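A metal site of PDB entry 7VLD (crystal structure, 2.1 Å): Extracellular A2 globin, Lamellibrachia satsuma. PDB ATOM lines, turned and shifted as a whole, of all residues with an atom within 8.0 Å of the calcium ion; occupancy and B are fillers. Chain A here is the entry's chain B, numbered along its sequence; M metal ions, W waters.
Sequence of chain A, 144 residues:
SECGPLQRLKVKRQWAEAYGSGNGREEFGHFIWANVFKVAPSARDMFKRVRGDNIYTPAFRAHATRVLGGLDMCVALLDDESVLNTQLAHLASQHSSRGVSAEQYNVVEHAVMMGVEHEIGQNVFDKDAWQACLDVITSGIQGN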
ATOM      1  N   ALA A 102       9.200 -36.669  -0.468  1.00  0.00           N
ATOM      2  CA  ALA A 102       8.822 -35.379  -1.032  1.00  0.00           C
ATOM      3  C   ALA A 102       7.606 -34.789  -0.321  1.00  0.00           C
ATOM      4  O   ALA A 102       7.484 -33.569  -0.206  1.00  0.00           O
ATOM      5  CB  ALA A 102       8.539 -35.521  -2.528  1.00  0.00           C
ATOM      6  N   GLU A 103       6.714 -35.650   0.165  1.00  0.00           N
ATOM      7  CA  GLU A 103       5.568 -35.181   0.947  1.00  0.00           C
ATOM      8  C   GLU A 103       6.013 -34.542   2.258  1.00  0.00           C
ATOM      9  O   GLU A 103       5.389 -33.590   2.728  1.00  0.00           O
ATOM     10  CB  GLU A 103       4.605 -36.332   1.219  1.00  0.00           C
ATOM     11  CG  GLU A 103       3.988 -36.976  -0.032  1.00  0.00           C
ATOM     12  CD  GLU A 103       4.939 -37.935  -0.747  1.00  0.00           C
ATOM     13  OE1 GLU A 103       6.093 -38.078  -0.314  1.00  0.00           O
ATOM     14  OE2 GLU A 103       4.513 -38.538  -1.759  1.00  0.00           O
ATOM     15  N   TYR A 105       8.969 -32.977   2.805  1.00  0.00           N
ATOM     16  CA  TYR A 105       9.552 -31.674   2.503  1.00  0.00           C
ATOM     17  C   TYR A 105       8.465 -30.618   2.318  1.00  0.00           C
ATOM     18  O   TYR A 105       8.635 -29.462   2.714  1.00  0.00           O
ATOM     19  CB  TYR A 105      10.444 -31.748   1.270  1.00  0.00           C
ATOM     20  CG  TYR A 105      11.832 -32.302   1.545  1.00  0.00           C
ATOM     21  CD1 TYR A 105      12.797 -31.530   2.176  1.00  0.00           C
ATOM     22  CD2 TYR A 105      12.178 -33.591   1.157  1.00  0.00           C
ATOM     23  CE1 TYR A 105      14.066 -32.028   2.425  1.00  0.00           C
ATOM     24  CE2 TYR A 105      13.442 -34.107   1.398  1.00  0.00           C
ATOM     25  CZ  TYR A 105      14.378 -33.320   2.038  1.00  0.00           C
ATOM     26  OH  TYR A 105      15.633 -33.821   2.278  1.00  0.00           O
ATOM     27  N   ASN A 106       7.329 -31.008   1.725  1.00  0.00           N
ATOM     28  CA  ASN A 106       6.227 -30.078   1.572  1.00  0.00           C
ATOM     29  C   ASN A 106       5.588 -29.724   2.910  1.00  0.00           C
ATOM     30  O   ASN A 106       5.122 -28.596   3.106  1.00  0.00           O
ATOM     31  CB  ASN A 106       5.171 -30.653   0.625  1.00  0.00           C
ATOM     32  CG  ASN A 106       5.693 -30.820  -0.800  1.00  0.00           C
ATOM     33  OD1 ASN A 106       6.657 -30.166  -1.203  1.00  0.00           O
ATOM     34  ND2 ASN A 106       5.049 -31.699  -1.559  1.00  0.00           N
ATOM     35  N   VAL A 107       5.576 -30.676   3.853  1.00  0.00           N
ATOM     36  CA  VAL A 107       5.026 -30.399   5.182  1.00  0.00           C
ATOM     37  C   VAL A 107       5.871 -29.352   5.903  1.00  0.00           C
ATOM     38  O   VAL A 107       5.339 -28.430   6.526  1.00  0.00           O
ATOM     39  CB  VAL A 107       4.913 -31.707   5.996  1.00  0.00           C
ATOM     40  CG1 VAL A 107       4.612 -31.410   7.452  1.00  0.00           C
ATOM     41  CG2 VAL A 107       3.844 -32.611   5.394  1.00  0.00           C
ATOM     42  N   GLU A 109       7.807 -27.205   4.374  1.00  0.00           N
ATOM     43  CA  GLU A 109       7.583 -25.985   3.603  1.00  0.00           C
ATOM     44  C   GLU A 109       6.393 -25.202   4.156  1.00  0.00           C
ATOM     45  O   GLU A 109       6.504 -24.002   4.443  1.00  0.00           O
ATOM     46  CB  GLU A 109       7.331 -26.325   2.125  1.00  0.00           C
ATOM     47  CG  GLU A 109       8.574 -26.652   1.298  1.00  0.00           C
ATOM     48  CD  GLU A 109       8.208 -27.076  -0.130  1.00  0.00           C
ATOM     49  OE1 GLU A 109       7.106 -26.738  -0.595  1.00  0.00           O
ATOM     50  OE2 GLU A 109       9.026 -27.755  -0.784  1.00  0.00           O
ATOM     51  N   HIS A 110       5.249 -25.876   4.316  1.00  0.00           N
ATOM     52  CA  HIS A 110       4.054 -25.196   4.799  1.00  0.00           C
ATOM     53  C   HIS A 110       4.234 -24.685   6.222  1.00  0.00           C
ATOM     54  O   HIS A 110       3.705 -23.635   6.573  1.00  0.00           O
ATOM     55  CB  HIS A 110       2.849 -26.137   4.717  1.00  0.00           C
ATOM     56  CG  HIS A 110       1.556 -25.504   5.139  1.00  0.00           C
ATOM     57  ND1 HIS A 110       0.980 -25.722   6.374  1.00  0.00           N
ATOM     58  CD2 HIS A 110       0.732 -24.648   4.476  1.00  0.00           C
ATOM     59  CE1 HIS A 110      -0.145 -25.034   6.460  1.00  0.00           C
ATOM     60  NE2 HIS A 110      -0.318 -24.383   5.321  1.00  0.00           N
ATOM     61  N   GLN A 131       6.343 -19.853  -1.651  1.00  0.00           N
ATOM     62  CA  GLN A 131       6.151 -21.209  -2.142  1.00  0.00           C
ATOM     63  C   GLN A 131       7.117 -21.529  -3.280  1.00  0.00           C
ATOM     64  O   GLN A 131       7.714 -22.608  -3.318  1.00  0.00           O
ATOM     65  CB  GLN A 131       4.706 -21.411  -2.591  1.00  0.00           C
ATOM     66  CG  GLN A 131       4.401 -22.828  -3.056  1.00  0.00           C
ATOM     67  CD  GLN A 131       4.627 -23.867  -1.970  1.00  0.00           C
ATOM     68  OE1 GLN A 131       5.659 -24.546  -1.949  1.00  0.00           O
ATOM     69  NE2 GLN A 131       3.668 -23.992  -1.073  1.00  0.00           N
ATOM     70  N   ALA A 132       7.288 -20.591  -4.213  1.00  0.00           N
ATOM     71  CA  ALA A 132       8.139 -20.838  -5.370  1.00  0.00           C
ATOM     72  C   ALA A 132       9.606 -20.968  -4.953  1.00  0.00           C
ATOM     73  O   ALA A 132      10.323 -21.844  -5.468  1.00  0.00           O
ATOM     74  CB  ALA A 132       7.972 -19.736  -6.407  1.00  0.00           C
ATOM     75  N   LEU A 134      10.841 -21.670  -1.852  1.00  0.00           N
ATOM     76  CA  LEU A 134      11.046 -22.863  -1.032  1.00  0.00           C
ATOM     77  C   LEU A 134      11.083 -24.117  -1.897  1.00  0.00           C
ATOM     78  O   LEU A 134      11.822 -25.063  -1.596  1.00  0.00           O
ATOM     79  CB  LEU A 134       9.954 -22.973   0.030  1.00  0.00           C
ATOM     80  CG  LEU A 134      10.116 -22.051   1.245  1.00  0.00           C
ATOM     81  CD1 LEU A 134       8.891 -22.134   2.134  1.00  0.00           C
ATOM     82  CD2 LEU A 134      11.368 -22.400   2.034  1.00  0.00           C
ATOM     83  N   ASP A 135      10.277 -24.146  -2.965  1.00  0.00           N
ATOM     84  CA  ASP A 135      10.359 -25.259  -3.915  1.00  0.00           C
ATOM     85  C   ASP A 135      11.755 -25.372  -4.509  1.00  0.00           C
ATOM     86  O   ASP A 135      12.276 -26.481  -4.681  1.00  0.00           O
ATOM     87  CB  ASP A 135       9.316 -25.081  -5.018  1.00  0.00           C
ATOM     88  CG  ASP A 135       7.911 -25.463  -4.575  1.00  0.00           C
ATOM     89  OD1 ASP A 135       7.787 -26.163  -3.546  1.00  0.00           O
ATOM     90  OD2 ASP A 135       6.950 -25.070  -5.265  1.00  0.00           O
ATOM     91  N   VAL A 136      12.371 -24.236  -4.838  1.00  0.00           N
ATOM     92  CA  VAL A 136      13.742 -24.254  -5.354  1.00  0.00           C
ATOM     93  C   VAL A 136      14.687 -24.851  -4.318  1.00  0.00           C
ATOM     94  O   VAL A 136      15.590 -25.632  -4.660  1.00  0.00           O
ATOM     95  CB  VAL A 136      14.179 -22.834  -5.772  1.00  0.00           C
ATOM     96  CG1 VAL A 136      15.666 -22.794  -6.044  1.00  0.00           C
ATOM     97  CG2 VAL A 136      13.393 -22.375  -6.995  1.00  0.00           C
ATOM     98  N   THR A 138      14.007 -26.926  -1.543  1.00  0.00           N
ATOM     99  CA  THR A 138      13.785 -28.318  -1.189  1.00  0.00           C
ATOM    100  C   THR A 138      14.088 -29.254  -2.353  1.00  0.00           C
ATOM    101  O   THR A 138      14.648 -30.341  -2.157  1.00  0.00           O
ATOM    102  CB  THR A 138      12.356 -28.534  -0.699  1.00  0.00           C
ATOM    103  OG1 THR A 138      11.431 -28.229  -1.754  1.00  0.00           O
ATOM    104  CG2 THR A 138      12.071 -27.657   0.509  1.00  0.00           C
ATOM    105  N   SER A 139      13.719 -28.864  -3.574  1.00  0.00           N
ATOM    106  CA  SER A 139      14.038 -29.702  -4.737  1.00  0.00           C
ATOM    107  C   SER A 139      15.539 -29.861  -4.909  1.00  0.00           C
ATOM    108  O   SER A 139      16.006 -30.896  -5.397  1.00  0.00           O
ATOM    109  CB  SER A 139      13.396 -29.139  -5.997  1.00  0.00           C
ATOM    110  OG  SER A 139      13.947 -27.865  -6.340  1.00  0.00           O
ATOM    111  N   GLN A 142      16.623 -32.409  -2.271  1.00  0.00           N
ATOM    112  CA  GLN A 142      16.252 -33.746  -2.723  1.00  0.00           C
ATOM    113  C   GLN A 142      17.101 -34.244  -3.877  1.00  0.00           C
ATOM    114  O   GLN A 142      16.726 -35.215  -4.547  1.00  0.00           O
ATOM    115  CB  GLN A 142      14.764 -33.767  -3.120  1.00  0.00           C
ATOM    116  CG  GLN A 142      13.826 -33.462  -1.966  1.00  0.00           C
ATOM    117  CD  GLN A 142      12.369 -33.503  -2.364  1.00  0.00           C
ATOM    118  OE1 GLN A 142      11.752 -34.568  -2.427  1.00  0.00           O
ATOM    119  NE2 GLN A 142      11.789 -32.328  -2.636  1.00  0.00           N
HETATM  120 CA    CA M   1       7.318 -28.245  -2.525  1.00  0.00          CA
HETATM  121  O   HOH W   1       4.944 -27.856  -2.361  1.00  0.00           O
HETATM  122  O   HOH W   2       6.416 -29.165  -4.694  1.00  0.00           O
HETATM  123  O   HOH W   3       9.292 -29.435  -3.199  1.00  0.00           O
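Of the 15 residues printed, 3 come within 4 Å of the calcium ion.
Along chain A the residues within 4 Å of the calcium ion span positions 106 to 135.
The side-chain hydroxyl (OG) of Ser 139 lies within hydrogen-bond range of the backbone carbonyl oxygen (O) of Asp 135, at 2.7 Å.
OD1 of Asp 135 lies close to OE1 of Gln 131 (3.1 Å).
OG1 of Thr 138 sits close to OE2 of Glu 109 (2.6 Å).
OE1 of Glu 109 sits close to OE1 of Gln 131, 3.0 Å away.
The side-chain amide nitrogen of Asn 106 lies close to the backbone carbonyl oxygen of Ala 102.
The calcium ion is bound by the side-chain carboxylate (OD1) of Asp 135 (2.4 Å), water W3 (2.4 Å), water W1 (2.4 Å), the side-chain amide oxygen (OD1) of Asn 106 (2.4 Å), the side-chain carboxylate (OE1) of Glu 109 (2.5 Å), the side-chain carboxylate (OE2) of Glu 109 (2.5 Å) and water W2 (2.5 Å).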
